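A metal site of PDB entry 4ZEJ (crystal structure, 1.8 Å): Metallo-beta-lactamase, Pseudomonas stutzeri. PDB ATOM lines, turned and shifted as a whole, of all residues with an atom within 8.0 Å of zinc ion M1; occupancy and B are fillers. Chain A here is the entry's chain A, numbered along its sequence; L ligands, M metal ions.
The side-chain carboxylate of Asp 80 lies within salt-bridge range of the guanidinium group of Arg 81 (3.9 Å).
O of Ser 31 sits at hydrogen-bond distance from ND1 of His 199 (2.7 Å).
The guanidinium group (NE) of Arg 81 sits close to the side-chain sulfur (SG) of Cys 157, 3.5 Å away.
NH2 of Arg 81 sits at hydrogen-bond distance from O of Gly 198 (3.3 Å).
OG of Ser 32 sits at hydrogen-bond distance from NH2 of Arg 81, 2.6 Å away.
The guanidinium group of Arg 81 sits at hydrogen-bond distance from the backbone carbonyl oxygen of Asn 33 (2.8 Å).
The guanidinium group of Arg 81 lies within salt-bridge range of the side-chain carboxylate of Asp 47 (2.8 Å).
NH2 of Arg 81 touches zinc ion M1, 3.9 Å away.
Four residues have an atom within 4 Å of zinc ion M1: Asp 80, Arg 81, Cys 157 and His 199.
Zinc ion M1 is bound by OD2 of Asp 80 (2.0 Å), NE2 of His 199 (2.1 Å), SG of Cys 157 (2.2 Å) and CL1 of LIG L1 (2.3 Å).
Slightly farther from zinc ion M1 lies a chlorine (CL1) of LG2 L2 (2.9 Å).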
ATOM      1  N   VAL A  30      22.268 -12.180 -28.000  1.00  0.00           N
ATOM      2  CA  VAL A  30      21.178 -13.132 -27.760  1.00  0.00           C
ATOM      3  C   VAL A  30      20.352 -12.662 -26.561  1.00  0.00           C
ATOM      4  O   VAL A  30      20.906 -12.368 -25.490  1.00  0.00           O
ATOM      5  CB  VAL A  30      21.708 -14.564 -27.538  1.00  0.00           C
ATOM      6  CG1 VAL A  30      20.563 -15.543 -27.212  1.00  0.00           C
ATOM      7  CG2 VAL A  30      22.451 -15.039 -28.774  1.00  0.00           C
ATOM      8  N   SER A  31      19.040 -12.561 -26.774  1.00  0.00           N
ATOM      9  CA  SER A  31      18.099 -12.254 -25.693  1.00  0.00           C
ATOM     10  C   SER A  31      17.715 -13.551 -24.952  1.00  0.00           C
ATOM     11  O   SER A  31      17.656 -14.625 -25.559  1.00  0.00           O
ATOM     12  CB  SER A  31      16.854 -11.568 -26.231  1.00  0.00           C
ATOM     13  OG  SER A  31      16.160 -12.418 -27.109  1.00  0.00           O
ATOM     14  N   SER A  32      17.468 -13.435 -23.671  1.00  0.00           N
ATOM     15  CA  SER A  32      17.190 -14.577 -22.806  1.00  0.00           C
ATOM     16  C   SER A  32      16.101 -14.200 -21.806  1.00  0.00           C
ATOM     17  O   SER A  32      16.123 -13.090 -21.268  1.00  0.00           O
ATOM     18  CB  SER A  32      18.468 -14.946 -22.052  1.00  0.00           C
ATOM     19  OG  SER A  32      18.263 -16.106 -21.306  1.00  0.00           O
ATOM     20  N   ASN A  33      15.156 -15.132 -21.560  1.00  0.00           N
ATOM     21  CA  ASN A  33      13.981 -14.900 -20.721  1.00  0.00           C
ATOM     22  C   ASN A  33      14.013 -15.655 -19.403  1.00  0.00           C
ATOM     23  O   ASN A  33      14.425 -16.816 -19.360  1.00  0.00           O
ATOM     24  CB  ASN A  33      12.723 -15.379 -21.446  1.00  0.00           C
ATOM     25  CG  ASN A  33      12.541 -14.734 -22.802  1.00  0.00           C
ATOM     26  OD1 ASN A  33      13.023 -13.627 -23.048  1.00  0.00           O
ATOM     27  ND2 ASN A  33      11.840 -15.428 -23.690  1.00  0.00           N
ATOM     28  N   ASP A  47      14.949 -18.760 -13.354  1.00  0.00           N
ATOM     29  CA  ASP A  47      16.167 -18.488 -14.128  1.00  0.00           C
ATOM     30  C   ASP A  47      16.777 -17.114 -13.893  1.00  0.00           C
ATOM     31  O   ASP A  47      16.080 -16.101 -13.832  1.00  0.00           O
ATOM     32  CB  ASP A  47      15.962 -18.777 -15.614  1.00  0.00           C
ATOM     33  CG  ASP A  47      15.822 -20.256 -15.900  1.00  0.00           C
ATOM     34  OD1 ASP A  47      16.484 -21.071 -15.219  1.00  0.00           O
ATOM     35  OD2 ASP A  47      15.108 -20.606 -16.859  1.00  0.00           O
ATOM     36  N   TRP A  50      21.573 -13.122 -17.387  1.00  0.00           N
ATOM     37  CA  TRP A  50      22.775 -13.664 -17.997  1.00  0.00           C
ATOM     38  C   TRP A  50      24.049 -12.970 -17.547  1.00  0.00           C
ATOM     39  O   TRP A  50      25.090 -13.168 -18.164  1.00  0.00           O
ATOM     40  CB  TRP A  50      22.608 -13.592 -19.520  1.00  0.00           C
ATOM     41  CG  TRP A  50      23.333 -14.622 -20.335  1.00  0.00           C
ATOM     42  CD1 TRP A  50      24.465 -15.338 -20.003  1.00  0.00           C
ATOM     43  CD2 TRP A  50      22.990 -15.016 -21.664  1.00  0.00           C
ATOM     44  NE1 TRP A  50      24.820 -16.165 -21.052  1.00  0.00           N
ATOM     45  CE2 TRP A  50      23.933 -15.984 -22.072  1.00  0.00           C
ATOM     46  CE3 TRP A  50      21.964 -14.645 -22.543  1.00  0.00           C
ATOM     47  CZ2 TRP A  50      23.887 -16.578 -23.333  1.00  0.00           C
ATOM     48  CZ3 TRP A  50      21.923 -15.233 -23.788  1.00  0.00           C
ATOM     49  CH2 TRP A  50      22.872 -16.198 -24.167  1.00  0.00           C
ATOM     50  N   THR A  75      16.585 -23.736 -14.712  1.00  0.00           N
ATOM     51  CA  THR A  75      15.886 -24.789 -15.472  1.00  0.00           C
ATOM     52  C   THR A  75      16.797 -25.674 -16.339  1.00  0.00           C
ATOM     53  O   THR A  75      16.356 -26.699 -16.835  1.00  0.00           O
ATOM     54  CB  THR A  75      14.733 -24.213 -16.318  1.00  0.00           C
ATOM     55  OG1 THR A  75      15.251 -23.250 -17.236  1.00  0.00           O
ATOM     56  CG2 THR A  75      13.682 -23.553 -15.407  1.00  0.00           C
ATOM     57  N   HIS A  76      18.044 -25.269 -16.528  1.00  0.00           N
ATOM     58  CA  HIS A  76      19.134 -26.200 -16.906  1.00  0.00           C
ATOM     59  C   HIS A  76      20.468 -25.525 -16.596  1.00  0.00           C
ATOM     60  O   HIS A  76      20.469 -24.408 -16.112  1.00  0.00           O
ATOM     61  CB  HIS A  76      19.037 -26.741 -18.361  1.00  0.00           C
ATOM     62  CG  HIS A  76      19.364 -25.755 -19.424  1.00  0.00           C
ATOM     63  ND1 HIS A  76      18.461 -24.796 -19.848  1.00  0.00           N
ATOM     64  CD2 HIS A  76      20.451 -25.598 -20.194  1.00  0.00           C
ATOM     65  CE1 HIS A  76      19.005 -24.085 -20.807  1.00  0.00           C
ATOM     66  NE2 HIS A  76      20.209 -24.544 -21.038  1.00  0.00           N
ATOM     67  N   HIS A  78      23.176 -24.315 -18.273  1.00  0.00           N
ATOM     68  CA  HIS A  78      23.915 -23.336 -19.077  1.00  0.00           C
ATOM     69  C   HIS A  78      23.834 -21.934 -18.497  1.00  0.00           C
ATOM     70  O   HIS A  78      22.921 -21.614 -17.735  1.00  0.00           O
ATOM     71  CB  HIS A  78      23.445 -23.332 -20.542  1.00  0.00           C
ATOM     72  CG  HIS A  78      23.802 -24.583 -21.283  1.00  0.00           C
ATOM     73  ND1 HIS A  78      23.089 -25.043 -22.367  1.00  0.00           N
ATOM     74  CD2 HIS A  78      24.788 -25.481 -21.078  1.00  0.00           C
ATOM     75  CE1 HIS A  78      23.643 -26.147 -22.826  1.00  0.00           C
ATOM     76  NE2 HIS A  78      24.668 -26.445 -22.055  1.00  0.00           N
ATOM     77  N   GLU A  79      24.795 -21.100 -18.895  1.00  0.00           N
ATOM     78  CA  GLU A  79      24.994 -19.775 -18.299  1.00  0.00           C
ATOM     79  C   GLU A  79      23.814 -18.816 -18.430  1.00  0.00           C
ATOM     80  O   GLU A  79      23.598 -17.970 -17.541  1.00  0.00           O
ATOM     81  CB  GLU A  79      26.254 -19.111 -18.869  1.00  0.00           C
ATOM     82  CG  GLU A  79      27.534 -19.757 -18.384  1.00  0.00           C
ATOM     83  CD  GLU A  79      28.795 -19.119 -18.939  1.00  0.00           C
ATOM     84  OE1 GLU A  79      28.772 -17.908 -19.297  1.00  0.00           O
ATOM     85  OE2 GLU A  79      29.829 -19.813 -19.007  1.00  0.00           O
ATOM     86  N   ASP A  80      23.038 -18.938 -19.509  1.00  0.00           N
ATOM     87  CA  ASP A  80      21.834 -18.089 -19.646  1.00  0.00           C
ATOM     88  C   ASP A  80      20.760 -18.389 -18.587  1.00  0.00           C
ATOM     89  O   ASP A  80      19.859 -17.581 -18.406  1.00  0.00           O
ATOM     90  CB  ASP A  80      21.243 -18.122 -21.072  1.00  0.00           C
ATOM     91  CG  ASP A  80      20.743 -19.485 -21.488  1.00  0.00           C
ATOM     92  OD1 ASP A  80      21.438 -20.473 -21.254  1.00  0.00           O
ATOM     93  OD2 ASP A  80      19.663 -19.575 -22.097  1.00  0.00           O
ATOM     94  N   ARG A  81      20.857 -19.525 -17.893  1.00  0.00           N
ATOM     95  CA  ARG A  81      19.942 -19.872 -16.786  1.00  0.00           C
ATOM     96  C   ARG A  81      20.534 -19.696 -15.374  1.00  0.00           C
ATOM     97  O   ARG A  81      19.781 -19.583 -14.395  1.00  0.00           O
ATOM     98  CB  ARG A  81      19.556 -21.352 -16.905  1.00  0.00           C
ATOM     99  CG  ARG A  81      19.085 -21.870 -18.241  1.00  0.00           C
ATOM    100  CD  ARG A  81      17.732 -21.318 -18.645  1.00  0.00           C
ATOM    101  NE  ARG A  81      17.856 -20.261 -19.616  1.00  0.00           N
ATOM    102  CZ  ARG A  81      16.921 -19.365 -19.920  1.00  0.00           C
ATOM    103  NH1 ARG A  81      15.726 -19.325 -19.301  1.00  0.00           N
ATOM    104  NH2 ARG A  81      17.182 -18.474 -20.859  1.00  0.00           N
ATOM    105  N   HIS A 138      16.690 -30.136 -25.149  1.00  0.00           N
ATOM    106  CA  HIS A 138      17.781 -29.200 -25.298  1.00  0.00           C
ATOM    107  C   HIS A 138      19.051 -29.697 -24.599  1.00  0.00           C
ATOM    108  O   HIS A 138      20.164 -29.587 -25.157  1.00  0.00           O
ATOM    109  CB  HIS A 138      17.366 -27.828 -24.751  1.00  0.00           C
ATOM    110  CG  HIS A 138      18.475 -26.848 -24.704  1.00  0.00           C
ATOM    111  ND1 HIS A 138      19.003 -26.293 -25.847  1.00  0.00           N
ATOM    112  CD2 HIS A 138      19.176 -26.331 -23.672  1.00  0.00           C
ATOM    113  CE1 HIS A 138      19.990 -25.489 -25.521  1.00  0.00           C
ATOM    114  NE2 HIS A 138      20.121 -25.500 -24.207  1.00  0.00           N
ATOM    115  N   GLY A 156      11.492 -22.742 -20.570  1.00  0.00           N
ATOM    116  CA  GLY A 156      12.923 -22.557 -20.699  1.00  0.00           C
ATOM    117  C   GLY A 156      13.369 -22.933 -22.104  1.00  0.00           C
ATOM    118  O   GLY A 156      12.594 -22.870 -23.065  1.00  0.00           O
ATOM    119  N   CYS A 157      14.619 -23.352 -22.229  1.00  0.00           N
ATOM    120  CA  CYS A 157      15.215 -23.585 -23.538  1.00  0.00           C
ATOM    121  C   CYS A 157      14.781 -24.928 -24.145  1.00  0.00           C
ATOM    122  O   CYS A 157      15.062 -25.219 -25.307  1.00  0.00           O
ATOM    123  CB  CYS A 157      16.717 -23.391 -23.439  1.00  0.00           C
ATOM    124  SG  CYS A 157      17.050 -21.809 -22.620  1.00  0.00           S
ATOM    125  N   PHE A 158      14.064 -25.728 -23.356  1.00  0.00           N
ATOM    126  CA  PHE A 158      13.324 -26.887 -23.860  1.00  0.00           C
ATOM    127  C   PHE A 158      12.219 -26.525 -24.886  1.00  0.00           C
ATOM    128  O   PHE A 158      11.825 -27.369 -25.703  1.00  0.00           O
ATOM    129  CB  PHE A 158      12.716 -27.639 -22.656  1.00  0.00           C
ATOM    130  CG  PHE A 158      11.890 -28.835 -23.008  1.00  0.00           C
ATOM    131  CD1 PHE A 158      10.502 -28.777 -22.998  1.00  0.00           C
ATOM    132  CD2 PHE A 158      12.493 -30.036 -23.332  1.00  0.00           C
ATOM    133  CE1 PHE A 158       9.743 -29.887 -23.308  1.00  0.00           C
ATOM    134  CE2 PHE A 158      11.743 -31.157 -23.660  1.00  0.00           C
ATOM    135  CZ  PHE A 158      10.369 -31.084 -23.641  1.00  0.00           C
ATOM    136  N   VAL A 159      11.707 -25.293 -24.810  1.00  0.00           N
ATOM    137  CA  VAL A 159      10.677 -24.798 -25.706  1.00  0.00           C
ATOM    138  C   VAL A 159      11.216 -23.667 -26.575  1.00  0.00           C
ATOM    139  O   VAL A 159      11.779 -22.693 -26.058  1.00  0.00           O
ATOM    140  CB  VAL A 159       9.442 -24.310 -24.901  1.00  0.00           C
ATOM    141  CG1 VAL A 159       8.370 -23.751 -25.823  1.00  0.00           C
ATOM    142  CG2 VAL A 159       8.878 -25.465 -24.084  1.00  0.00           C
ATOM    143  N   ARG A 160      11.008 -23.791 -27.882  1.00  0.00           N
ATOM    144  CA  ARG A 160      11.393 -22.787 -28.866  1.00  0.00           C
ATOM    145  C   ARG A 160      10.231 -21.855 -29.192  1.00  0.00           C
ATOM    146  O   ARG A 160       9.054 -22.253 -29.139  1.00  0.00           O
ATOM    147  CB  ARG A 160      11.894 -23.455 -30.149  1.00  0.00           C
ATOM    148  CG  ARG A 160      12.999 -24.476 -29.930  1.00  0.00           C
ATOM    149  CD  ARG A 160      14.304 -23.817 -29.527  1.00  0.00           C
ATOM    150  NE  ARG A 160      14.821 -23.025 -30.640  1.00  0.00           N
ATOM    151  CZ  ARG A 160      15.807 -22.136 -30.550  1.00  0.00           C
ATOM    152  NH1 ARG A 160      16.443 -21.889 -29.388  1.00  0.00           N
ATOM    153  NH2 ARG A 160      16.171 -21.505 -31.648  1.00  0.00           N
ATOM    154  N   TYR A 169      21.199 -24.077 -30.152  1.00  0.00           N
ATOM    155  CA  TYR A 169      22.437 -24.833 -29.875  1.00  0.00           C
ATOM    156  C   TYR A 169      22.095 -26.290 -29.550  1.00  0.00           C
ATOM    157  O   TYR A 169      21.439 -26.546 -28.535  1.00  0.00           O
ATOM    158  CB  TYR A 169      23.217 -24.197 -28.709  1.00  0.00           C
ATOM    159  CG  TYR A 169      24.369 -25.076 -28.233  1.00  0.00           C
ATOM    160  CD1 TYR A 169      25.495 -25.276 -29.025  1.00  0.00           C
ATOM    161  CD2 TYR A 169      24.312 -25.716 -27.006  1.00  0.00           C
ATOM    162  CE1 TYR A 169      26.553 -26.079 -28.589  1.00  0.00           C
ATOM    163  CE2 TYR A 169      25.347 -26.523 -26.561  1.00  0.00           C
ATOM    164  CZ  TYR A 169      26.466 -26.700 -27.348  1.00  0.00           C
ATOM    165  OH  TYR A 169      27.486 -27.514 -26.889  1.00  0.00           O
ATOM    166  N   PRO A 197       9.058 -19.396 -23.730  1.00  0.00           N
ATOM    167  CA  PRO A 197      10.323 -20.009 -24.136  1.00  0.00           C
ATOM    168  C   PRO A 197      11.511 -19.346 -23.445  1.00  0.00           C
ATOM    169  O   PRO A 197      11.406 -18.234 -22.953  1.00  0.00           O
ATOM    170  CB  PRO A 197      10.364 -19.736 -25.650  1.00  0.00           C
ATOM    171  CG  PRO A 197       9.705 -18.412 -25.780  1.00  0.00           C
ATOM    172  CD  PRO A 197       8.625 -18.384 -24.724  1.00  0.00           C
ATOM    173  N   GLY A 198      12.657 -20.044 -23.430  1.00  0.00           N
ATOM    174  CA  GLY A 198      13.893 -19.508 -22.915  1.00  0.00           C
ATOM    175  C   GLY A 198      14.385 -18.307 -23.715  1.00  0.00           C
ATOM    176  O   GLY A 198      15.036 -17.434 -23.184  1.00  0.00           O
ATOM    177  N   HIS A 199      14.061 -18.291 -25.010  1.00  0.00           N
ATOM    178  CA  HIS A 199      14.490 -17.220 -25.918  1.00  0.00           C
ATOM    179  C   HIS A 199      13.351 -16.881 -26.866  1.00  0.00           C
ATOM    180  O   HIS A 199      12.734 -17.774 -27.419  1.00  0.00           O
ATOM    181  CB  HIS A 199      15.682 -17.688 -26.744  1.00  0.00           C
ATOM    182  CG  HIS A 199      16.830 -18.162 -25.913  1.00  0.00           C
ATOM    183  ND1 HIS A 199      17.730 -17.294 -25.333  1.00  0.00           N
ATOM    184  CD2 HIS A 199      17.193 -19.407 -25.535  1.00  0.00           C
ATOM    185  CE1 HIS A 199      18.617 -17.990 -24.648  1.00  0.00           C
ATOM    186  NE2 HIS A 199      18.323 -19.280 -24.756  1.00  0.00           N
HETATM  187 CL1  LIG L   1      20.688 -22.222 -23.544  1.00  0.00          CL
HETATM  188 CL1  LG2 L   2      18.911 -22.143 -26.005  1.00  0.00          CL
HETATM  189 ZN    ZN M   1      18.863 -20.879 -23.432  1.00  0.00          ZN
HETATM  190 ZN    ZN M   2      21.248 -24.324 -22.916  1.00  0.00          ZN
